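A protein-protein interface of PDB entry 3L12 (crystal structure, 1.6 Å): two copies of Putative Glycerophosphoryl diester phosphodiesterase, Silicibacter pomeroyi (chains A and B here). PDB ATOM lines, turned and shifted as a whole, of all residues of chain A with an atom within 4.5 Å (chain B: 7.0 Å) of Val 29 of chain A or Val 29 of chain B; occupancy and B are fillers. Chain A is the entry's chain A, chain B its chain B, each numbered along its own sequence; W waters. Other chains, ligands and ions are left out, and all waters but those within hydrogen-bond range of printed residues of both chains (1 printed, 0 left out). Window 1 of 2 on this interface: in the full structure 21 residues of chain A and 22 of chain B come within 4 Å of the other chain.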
ATOM      1  N   ALA A  26     -18.768  -0.139 -26.426  1.00  0.00           N
ATOM      2  CA  ALA A  26     -19.175  -1.436 -25.863  1.00  0.00           C
ATOM      3  C   ALA A  26     -17.888  -2.219 -25.619  1.00  0.00           C
ATOM      4  O   ALA A  26     -17.574  -3.134 -26.347  1.00  0.00           O
ATOM      5  CB  ALA A  26     -20.051  -2.190 -26.779  1.00  0.00           C
ATOM      6  N   ARG A  27     -17.136  -1.797 -24.611  1.00  0.00           N
ATOM      7  CA  ARG A  27     -15.842  -2.379 -24.321  1.00  0.00           C
ATOM      8  C   ARG A  27     -15.872  -3.899 -24.135  1.00  0.00           C
ATOM      9  O   ARG A  27     -14.899  -4.591 -24.395  1.00  0.00           O
ATOM     10  CB  ARG A  27     -15.254  -1.677 -23.093  1.00  0.00           C
ATOM     11  CG  ARG A  27     -13.952  -2.283 -22.528  1.00  0.00           C
ATOM     12  CD  ARG A  27     -13.287  -1.427 -21.469  1.00  0.00           C
ATOM     13  NE  ARG A  27     -14.133  -1.228 -20.277  1.00  0.00           N
ATOM     14  CZ  ARG A  27     -13.723  -0.851 -19.096  1.00  0.00           C
ATOM     15  NH1 ARG A  27     -12.435  -0.595 -18.846  1.00  0.00           N
ATOM     16  NH2 ARG A  27     -14.593  -0.779 -18.096  1.00  0.00           N
ATOM     17  N   GLY A  28     -16.957  -4.472 -23.632  1.00  0.00           N
ATOM     18  CA  GLY A  28     -17.020  -5.944 -23.579  1.00  0.00           C
ATOM     19  C   GLY A  28     -17.098  -6.682 -24.902  1.00  0.00           C
ATOM     20  O   GLY A  28     -16.838  -7.880 -24.929  1.00  0.00           O
ATOM     21  N   VAL A  29     -17.453  -5.994 -26.004  1.00  0.00           N
ATOM     22  CA  VAL A  29     -17.689  -6.553 -27.320  1.00  0.00           C
ATOM     23  C   VAL A  29     -16.655  -6.118 -28.419  1.00  0.00           C
ATOM     24  O   VAL A  29     -16.243  -6.905 -29.241  1.00  0.00           O
ATOM     25  CB  VAL A  29     -19.143  -6.226 -27.826  1.00  0.00           C
ATOM     26  CG1 VAL A  29     -19.443  -7.001 -29.140  1.00  0.00           C
ATOM     27  CG2 VAL A  29     -20.179  -6.520 -26.673  1.00  0.00           C
ATOM     28  N   MET A  30     -16.284  -4.844 -28.399  1.00  0.00           N
ATOM     29  CA  MET A  30     -15.431  -4.226 -29.335  1.00  0.00           C
ATOM     30  C   MET A  30     -14.367  -3.391 -28.647  1.00  0.00           C
ATOM     31  O   MET A  30     -14.567  -2.943 -27.568  1.00  0.00           O
ATOM     32  CB  MET A  30     -16.231  -3.280 -30.243  1.00  0.00           C
ATOM     33  CG  MET A  30     -17.104  -4.080 -31.192  1.00  0.00           C
ATOM     34  SD  MET A  30     -16.289  -5.041 -32.628  1.00  0.00           S
ATOM     35  CE  MET A  30     -16.053  -3.535 -33.842  1.00  0.00           C
ATOM     36  N   PHE A  40     -20.742  -0.132 -33.806  1.00  0.00           N
ATOM     37  CA  PHE A  40     -21.363  -1.356 -33.347  1.00  0.00           C
ATOM     38  C   PHE A  40     -22.436  -1.032 -32.253  1.00  0.00           C
ATOM     39  O   PHE A  40     -23.581  -1.530 -32.292  1.00  0.00           O
ATOM     40  CB  PHE A  40     -20.352  -2.323 -32.709  1.00  0.00           C
ATOM     41  CG  PHE A  40     -21.034  -3.302 -31.763  1.00  0.00           C
ATOM     42  CD1 PHE A  40     -21.868  -4.274 -32.307  1.00  0.00           C
ATOM     43  CD2 PHE A  40     -20.961  -3.174 -30.364  1.00  0.00           C
ATOM     44  CE1 PHE A  40     -22.573  -5.155 -31.492  1.00  0.00           C
ATOM     45  CE2 PHE A  40     -21.676  -4.044 -29.569  1.00  0.00           C
ATOM     46  CZ  PHE A  40     -22.477  -5.031 -30.140  1.00  0.00           C
ATOM     47  N   ASP A 117     -13.958 -11.701 -24.415  1.00  0.00           N
ATOM     48  CA  ASP A 117     -14.796 -11.924 -25.556  1.00  0.00           C
ATOM     49  C   ASP A 117     -14.815 -10.780 -26.559  1.00  0.00           C
ATOM     50  O   ASP A 117     -15.443 -10.857 -27.627  1.00  0.00           O
ATOM     51  CB  ASP A 117     -16.218 -12.212 -25.085  1.00  0.00           C
ATOM     52  CG  ASP A 117     -16.354 -13.525 -24.332  1.00  0.00           C
ATOM     53  OD1 ASP A 117     -15.417 -14.363 -24.212  1.00  0.00           O
ATOM     54  OD2 ASP A 117     -17.508 -13.659 -23.849  1.00  0.00           O
ATOM     55  N   GLN A 118     -14.001  -9.768 -26.313  1.00  0.00           N
ATOM     56  CA  GLN A 118     -13.913  -8.605 -27.164  1.00  0.00           C
ATOM     57  C   GLN A 118     -13.225  -9.005 -28.460  1.00  0.00           C
ATOM     58  O   GLN A 118     -12.189  -9.660 -28.427  1.00  0.00           O
ATOM     59  CB  GLN A 118     -13.099  -7.521 -26.444  1.00  0.00           C
ATOM     60  CG  GLN A 118     -12.938  -6.249 -27.266  1.00  0.00           C
ATOM     61  CD  GLN A 118     -11.928  -5.310 -26.639  1.00  0.00           C
ATOM     62  OE1 GLN A 118     -10.812  -5.267 -27.110  1.00  0.00           O
ATOM     63  NE2 GLN A 118     -12.347  -4.468 -25.655  1.00  0.00           N
ATOM     64  N   ALA A 119     -13.782  -8.586 -29.582  1.00  0.00           N
ATOM     65  CA  ALA A 119     -13.185  -8.804 -30.876  1.00  0.00           C
ATOM     66  C   ALA A 119     -11.772  -8.250 -30.927  1.00  0.00           C
ATOM     67  O   ALA A 119     -11.455  -7.282 -30.253  1.00  0.00           O
ATOM     68  CB  ALA A 119     -14.023  -8.174 -31.979  1.00  0.00           C
ATOM     69  N   ASP A 296     -20.311  -1.916 -19.902  1.00  0.00           N
ATOM     70  CA  ASP A 296     -19.468  -2.504 -20.922  1.00  0.00           C
ATOM     71  C   ASP A 296     -20.190  -3.548 -21.804  1.00  0.00           C
ATOM     72  O   ASP A 296     -19.684  -3.938 -22.882  1.00  0.00           O
ATOM     73  CB  ASP A 296     -18.251  -3.196 -20.268  1.00  0.00           C
ATOM     74  CG  ASP A 296     -17.323  -2.205 -19.566  1.00  0.00           C
ATOM     75  OD1 ASP A 296     -17.031  -1.183 -20.164  1.00  0.00           O
ATOM     76  OD2 ASP A 296     -16.868  -2.481 -18.441  1.00  0.00           O
ATOM     77  N   ALA B  26     -23.237 -14.103 -35.551  1.00  0.00           N
ATOM     78  CA  ALA B  26     -22.653 -14.188 -34.230  1.00  0.00           C
ATOM     79  C   ALA B  26     -23.788 -14.254 -33.190  1.00  0.00           C
ATOM     80  O   ALA B  26     -24.048 -13.297 -32.477  1.00  0.00           O
ATOM     81  CB  ALA B  26     -21.737 -12.998 -33.988  1.00  0.00           C
ATOM     82  N   ARG B  27     -24.398 -15.434 -33.090  1.00  0.00           N
ATOM     83  CA  ARG B  27     -25.578 -15.641 -32.275  1.00  0.00           C
ATOM     84  C   ARG B  27     -25.380 -15.291 -30.835  1.00  0.00           C
ATOM     85  O   ARG B  27     -26.289 -14.831 -30.160  1.00  0.00           O
ATOM     86  CB  ARG B  27     -26.092 -17.074 -32.470  1.00  0.00           C
ATOM     87  CG  ARG B  27     -27.150 -17.498 -31.528  1.00  0.00           C
ATOM     88  CD  ARG B  27     -27.756 -18.868 -31.855  1.00  0.00           C
ATOM     89  NE  ARG B  27     -26.760 -19.951 -31.782  1.00  0.00           N
ATOM     90  CZ  ARG B  27     -27.041 -21.224 -31.587  1.00  0.00           C
ATOM     91  NH1 ARG B  27     -28.307 -21.663 -31.481  1.00  0.00           N
ATOM     92  NH2 ARG B  27     -26.031 -22.084 -31.483  1.00  0.00           N
ATOM     93  N   GLY B  28     -24.158 -15.416 -30.353  1.00  0.00           N
ATOM     94  CA  GLY B  28     -23.885 -15.038 -28.987  1.00  0.00           C
ATOM     95  C   GLY B  28     -23.940 -13.565 -28.656  1.00  0.00           C
ATOM     96  O   GLY B  28     -24.111 -13.186 -27.501  1.00  0.00           O
ATOM     97  N   VAL B  29     -23.838 -12.725 -29.665  1.00  0.00           N
ATOM     98  CA  VAL B  29     -23.771 -11.244 -29.566  1.00  0.00           C
ATOM     99  C   VAL B  29     -24.962 -10.482 -30.167  1.00  0.00           C
ATOM    100  O   VAL B  29     -25.384  -9.463 -29.627  1.00  0.00           O
ATOM    101  CB  VAL B  29     -22.471 -10.735 -30.240  1.00  0.00           C
ATOM    102  CG1 VAL B  29     -22.264  -9.275 -30.004  1.00  0.00           C
ATOM    103  CG2 VAL B  29     -21.219 -11.559 -29.720  1.00  0.00           C
ATOM    104  N   MET B  30     -25.447 -10.970 -31.305  1.00  0.00           N
ATOM    105  CA  MET B  30     -26.532 -10.367 -32.022  1.00  0.00           C
ATOM    106  C   MET B  30     -27.551 -11.391 -32.433  1.00  0.00           C
ATOM    107  O   MET B  30     -27.202 -12.551 -32.630  1.00  0.00           O
ATOM    108  CB  MET B  30     -25.941  -9.711 -33.280  1.00  0.00           C
ATOM    109  CG  MET B  30     -25.093  -8.471 -32.967  1.00  0.00           C
ATOM    110  SD  MET B  30     -26.014  -6.940 -32.384  1.00  0.00           S
ATOM    111  CE  MET B  30     -26.512  -6.188 -34.021  1.00  0.00           C
ATOM    112  N   PRO B  31     -28.821 -10.978 -32.603  1.00  0.00           N
ATOM    113  CA  PRO B  31     -29.831 -11.946 -33.051  1.00  0.00           C
ATOM    114  C   PRO B  31     -29.371 -12.698 -34.291  1.00  0.00           C
ATOM    115  O   PRO B  31     -28.850 -12.158 -35.271  1.00  0.00           O
ATOM    116  CB  PRO B  31     -31.079 -11.096 -33.338  1.00  0.00           C
ATOM    117  CG  PRO B  31     -30.565  -9.684 -33.468  1.00  0.00           C
ATOM    118  CD  PRO B  31     -29.360  -9.621 -32.518  1.00  0.00           C
ATOM    119  N   GLY B  37     -26.769  -8.738 -37.487  1.00  0.00           N
ATOM    120  CA  GLY B  37     -25.771  -9.679 -36.937  1.00  0.00           C
ATOM    121  C   GLY B  37     -24.663  -9.957 -37.929  1.00  0.00           C
ATOM    122  O   GLY B  37     -23.518 -10.061 -37.546  1.00  0.00           O
ATOM    123  N   PHE B  40     -22.373  -6.959 -38.039  1.00  0.00           N
ATOM    124  CA  PHE B  40     -21.526  -6.943 -36.872  1.00  0.00           C
ATOM    125  C   PHE B  40     -20.370  -7.910 -37.045  1.00  0.00           C
ATOM    126  O   PHE B  40     -19.229  -7.573 -36.749  1.00  0.00           O
ATOM    127  CB  PHE B  40     -22.281  -7.342 -35.592  1.00  0.00           C
ATOM    128  CG  PHE B  40     -21.358  -7.798 -34.507  1.00  0.00           C
ATOM    129  CD1 PHE B  40     -20.529  -6.911 -33.879  1.00  0.00           C
ATOM    130  CD2 PHE B  40     -21.256  -9.142 -34.216  1.00  0.00           C
ATOM    131  CE1 PHE B  40     -19.624  -7.387 -32.884  1.00  0.00           C
ATOM    132  CE2 PHE B  40     -20.342  -9.615 -33.314  1.00  0.00           C
ATOM    133  CZ  PHE B  40     -19.527  -8.691 -32.614  1.00  0.00           C
ATOM    134  N   ALA B  44     -16.368  -7.145 -37.010  1.00  0.00           N
ATOM    135  CA  ALA B  44     -15.480  -7.775 -35.997  1.00  0.00           C
ATOM    136  C   ALA B  44     -14.278  -8.454 -36.642  1.00  0.00           C
ATOM    137  O   ALA B  44     -13.478  -9.097 -35.997  1.00  0.00           O
ATOM    138  CB  ALA B  44     -16.260  -8.715 -35.110  1.00  0.00           C
ATOM    139  N   PHE B 115     -28.397 -17.570 -24.399  1.00  0.00           N
ATOM    140  CA  PHE B 115     -27.714 -16.381 -24.995  1.00  0.00           C
ATOM    141  C   PHE B 115     -28.175 -15.096 -24.323  1.00  0.00           C
ATOM    142  O   PHE B 115     -28.775 -14.201 -24.977  1.00  0.00           O
ATOM    143  CB  PHE B 115     -27.941 -16.332 -26.509  1.00  0.00           C
ATOM    144  CG  PHE B 115     -27.614 -17.628 -27.196  1.00  0.00           C
ATOM    145  CD1 PHE B 115     -26.305 -18.017 -27.364  1.00  0.00           C
ATOM    146  CD2 PHE B 115     -28.613 -18.447 -27.653  1.00  0.00           C
ATOM    147  CE1 PHE B 115     -25.985 -19.231 -27.951  1.00  0.00           C
ATOM    148  CE2 PHE B 115     -28.293 -19.655 -28.319  1.00  0.00           C
ATOM    149  CZ  PHE B 115     -26.976 -20.038 -28.448  1.00  0.00           C
ATOM    150  N   ASP B 117     -26.524 -12.543 -23.244  1.00  0.00           N
ATOM    151  CA  ASP B 117     -25.784 -11.280 -23.517  1.00  0.00           C
ATOM    152  C   ASP B 117     -26.050 -10.760 -24.917  1.00  0.00           C
ATOM    153  O   ASP B 117     -25.515  -9.742 -25.339  1.00  0.00           O
ATOM    154  CB  ASP B 117     -24.303 -11.522 -23.329  1.00  0.00           C
ATOM    155  CG  ASP B 117     -23.954 -11.884 -21.905  1.00  0.00           C
ATOM    156  OD1 ASP B 117     -24.759 -11.646 -21.017  1.00  0.00           O
ATOM    157  OD2 ASP B 117     -22.844 -12.387 -21.728  1.00  0.00           O
ATOM    158  N   GLN B 118     -26.884 -11.485 -25.678  1.00  0.00           N
ATOM    159  CA  GLN B 118     -27.250 -11.040 -27.000  1.00  0.00           C
ATOM    160  C   GLN B 118     -28.047  -9.732 -26.940  1.00  0.00           C
ATOM    161  O   GLN B 118     -29.011  -9.612 -26.171  1.00  0.00           O
ATOM    162  CB  GLN B 118     -28.112 -12.117 -27.686  1.00  0.00           C
ATOM    163  CG  GLN B 118     -28.418 -11.926 -29.155  1.00  0.00           C
ATOM    164  CD  GLN B 118     -29.442 -12.918 -29.663  1.00  0.00           C
ATOM    165  OE1 GLN B 118     -30.671 -12.651 -29.630  1.00  0.00           O
ATOM    166  NE2 GLN B 118     -28.961 -14.068 -30.196  1.00  0.00           N
ATOM    167  N   ALA B 119     -27.753  -8.817 -27.866  1.00  0.00           N
ATOM    168  CA  ALA B 119     -28.523  -7.573 -27.928  1.00  0.00           C
ATOM    169  C   ALA B 119     -30.006  -7.869 -28.246  1.00  0.00           C
ATOM    170  O   ALA B 119     -30.344  -8.855 -28.874  1.00  0.00           O
ATOM    171  CB  ALA B 119     -27.998  -6.679 -29.068  1.00  0.00           C
ATOM    172  N   PHE B 120     -30.859  -6.975 -27.775  1.00  0.00           N
ATOM    173  CA  PHE B 120     -32.297  -7.112 -27.932  1.00  0.00           C
ATOM    174  C   PHE B 120     -32.768  -5.985 -28.855  1.00  0.00           C
ATOM    175  O   PHE B 120     -32.960  -4.844 -28.410  1.00  0.00           O
ATOM    176  CB  PHE B 120     -33.011  -7.047 -26.620  1.00  0.00           C
ATOM    177  CG  PHE B 120     -34.454  -7.437 -26.725  1.00  0.00           C
ATOM    178  CD1 PHE B 120     -34.813  -8.793 -26.641  1.00  0.00           C
ATOM    179  CD2 PHE B 120     -35.459  -6.501 -26.946  1.00  0.00           C
ATOM    180  CE1 PHE B 120     -36.111  -9.182 -26.789  1.00  0.00           C
ATOM    181  CE2 PHE B 120     -36.791  -6.909 -27.085  1.00  0.00           C
ATOM    182  CZ  PHE B 120     -37.140  -8.237 -26.993  1.00  0.00           C
ATOM    183  N   LEU B 121     -32.941  -6.308 -30.122  1.00  0.00           N
ATOM    184  CA  LEU B 121     -33.365  -5.343 -31.132  1.00  0.00           C
ATOM    185  C   LEU B 121     -34.838  -5.530 -31.410  1.00  0.00           C
ATOM    186  O   LEU B 121     -35.415  -6.583 -31.118  1.00  0.00           O
ATOM    187  CB  LEU B 121     -32.549  -5.521 -32.415  1.00  0.00           C
ATOM    188  CG  LEU B 121     -31.079  -5.050 -32.471  1.00  0.00           C
ATOM    189  CD1 LEU B 121     -30.207  -5.731 -31.420  1.00  0.00           C
ATOM    190  CD2 LEU B 121     -30.527  -5.336 -33.868  1.00  0.00           C
ATOM    191  N   ASP B 296     -20.465 -19.414 -32.078  1.00  0.00           N
ATOM    192  CA  ASP B 296     -21.418 -18.372 -31.723  1.00  0.00           C
ATOM    193  C   ASP B 296     -20.727 -17.116 -31.143  1.00  0.00           C
ATOM    194  O   ASP B 296     -21.339 -16.062 -31.048  1.00  0.00           O
ATOM    195  CB  ASP B 296     -22.464 -18.875 -30.718  1.00  0.00           C
ATOM    196  CG  ASP B 296     -23.406 -19.939 -31.298  1.00  0.00           C
ATOM    197  OD1 ASP B 296     -23.969 -19.645 -32.374  1.00  0.00           O
ATOM    198  OD2 ASP B 296     -23.623 -20.944 -30.618  1.00  0.00           O
ATOM    199  N   TYR B 297     -19.427 -17.216 -30.837  1.00  0.00           N
ATOM    200  CA  TYR B 297     -18.666 -16.151 -30.167  1.00  0.00           C
ATOM    201  C   TYR B 297     -17.351 -15.893 -30.916  1.00  0.00           C
ATOM    202  O   TYR B 297     -16.268 -16.317 -30.503  1.00  0.00           O
ATOM    203  CB  TYR B 297     -18.380 -16.513 -28.691  1.00  0.00           C
ATOM    204  CG  TYR B 297     -19.647 -16.765 -27.914  1.00  0.00           C
ATOM    205  CD1 TYR B 297     -20.231 -15.748 -27.223  1.00  0.00           C
ATOM    206  CD2 TYR B 297     -20.250 -18.030 -27.893  1.00  0.00           C
ATOM    207  CE1 TYR B 297     -21.389 -15.928 -26.524  1.00  0.00           C
ATOM    208  CE2 TYR B 297     -21.431 -18.227 -27.156  1.00  0.00           C
ATOM    209  CZ  TYR B 297     -21.975 -17.172 -26.486  1.00  0.00           C
ATOM    210  OH  TYR B 297     -23.145 -17.363 -25.717  1.00  0.00           O
ATOM    211  N   PRO B 298     -17.427 -15.176 -32.039  1.00  0.00           N
ATOM    212  CA  PRO B 298     -16.217 -14.983 -32.831  1.00  0.00           C
ATOM    213  C   PRO B 298     -15.076 -14.237 -32.124  1.00  0.00           C
ATOM    214  O   PRO B 298     -13.875 -14.627 -32.307  1.00  0.00           O
ATOM    215  CB  PRO B 298     -16.719 -14.230 -34.066  1.00  0.00           C
ATOM    216  CG  PRO B 298     -18.132 -14.334 -34.085  1.00  0.00           C
ATOM    217  CD  PRO B 298     -18.630 -14.682 -32.736  1.00  0.00           C
ATOM    218  N   GLY B 299     -15.413 -13.217 -31.310  1.00  0.00           N
ATOM    219  CA  GLY B 299     -14.401 -12.473 -30.579  1.00  0.00           C
ATOM    220  C   GLY B 299     -13.697 -13.352 -29.569  1.00  0.00           C
ATOM    221  O   GLY B 299     -12.444 -13.328 -29.427  1.00  0.00           O
HETATM  222  O   HOH W   1     -18.291  -5.256 -35.315  1.00  0.00           O
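Val 29 of chain B touches its own counterpart, Val 29 of chain A. Val 29 of chain A touches Phe 40 of chain B, but with the chains exchanged Phe 40 of chain A does not touch Val 29 of chain B (4.3 Å). Phe 40 of chain A touches Met 30 of chain B, but with the chains exchanged Met 30 of chain A does not touch Phe 40 of chain B (4.1 Å). Phe 40 of chain B touches its own counterpart, Phe 40 of chain A. 10 positions are printed for both chains. Of the 8 pairs that touch across the chains among the printed residues, 2 have their exchanged pair printed and touching as well.
Water W1 lies within hydrogen-bond range of O of Phe 40 of chain B (2.9 Å), N of Ala 44 of chain B (3.2 Å) and SD of Met 30 of chain A (3.4 Å).
CG1 of Val 29 of chain B touches CG1 of Val 29 of chain A, 3.7 Å away. Val 29 of chain A touches Phe 40 of chain B. Met 30 of chain B touches Phe 40 of chain A (SD to CE1, 3.98 Å). CD1 of Phe 40 of chain A touches CD1 of Phe 40 of chain B, at 3.3 Å. Gly 299 of chain B touches Asp 117 of chain A (CA to O, 3.5 Å). Gln 118 of chain A touches Gly 299 of chain B. Ala 44 of chain B touches Ala 119 of chain A. Gly 299 of chain B touches Ala 119 of chain A.
Ala 26 of chain A touches none of the printed residues of chain B. No residue of chain B comes within 4 Å of Gly 28 of chain A. Val 29 of chain A touches just these residues of chain B: Val 29 (3.7 Å) and Phe 40 (3.8 Å). Of the printed residues of chain B, Phe 40 of chain A touches Met 30 (3.98 Å) and Phe 40 (3.3 Å). Printed residues of chain B within 4 Å of Gln 118 of chain A: Gly 299. Printed residues of chain B within 4 Å of Ala 119 of chain A: Ala 44 and Gly 299. Val 29 of chain B touches one residue of chain A. Printed residues of chain A within 4 Å of Phe 40 of chain B: Val 29 (3.8 Å) and Phe 40 (3.3 Å). Of the printed residues of chain A, Ala 44 of chain B touches Ala 119. Gln 118 of chain B touches none of the printed residues of chain A. The nearest residue of chain B that does not touch Val 29 of chain A is Gly 299 of chain B (6.0 Å). The nearest printed residue of chain B that does not touch Phe 40 of chain A is Val 29 of chain B (4.3 Å).
The backbone carbonyl oxygen (O) of Val 29 of chain B sits at hydrogen-bond distance from the backbone NH (N) of Ala 119 of chain B (3.0 Å). The backbone carbonyl oxygen (O) of Arg 27 of chain A lies within hydrogen-bond range of the side-chain amide nitrogen (NE2) of Gln 118 of chain A. O of Met 30 of chain A is in hydrogen-bond range of NE2 of Gln 118 of chain A. N of Ala 119 of chain A is in hydrogen-bond range of O of Val 29 of chain A, at 3.0 Å. The backbone carbonyl oxygen (O) of Met 30 of chain B is in hydrogen-bond range of the side-chain amide nitrogen (NE2) of Gln 118 of chain B, 3.4 Å away.
Hydrophobic or aromatic side chains of chain B within 4 Å of the printed part of chain A: Val 29, Met 30, Phe 40 and Ala 44. Hydrophobic or aromatic side chains of chain A within 4 Å of the printed part of chain B: Val 29, Phe 40 and Ala 119. Along chain A the printed residues that touch a printed residue of chain B span positions 29 to 119. Among the printed residues, no Asp or Glu carboxylate lies within 4 Å of a Lys or Arg side-chain nitrogen of the other chain.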
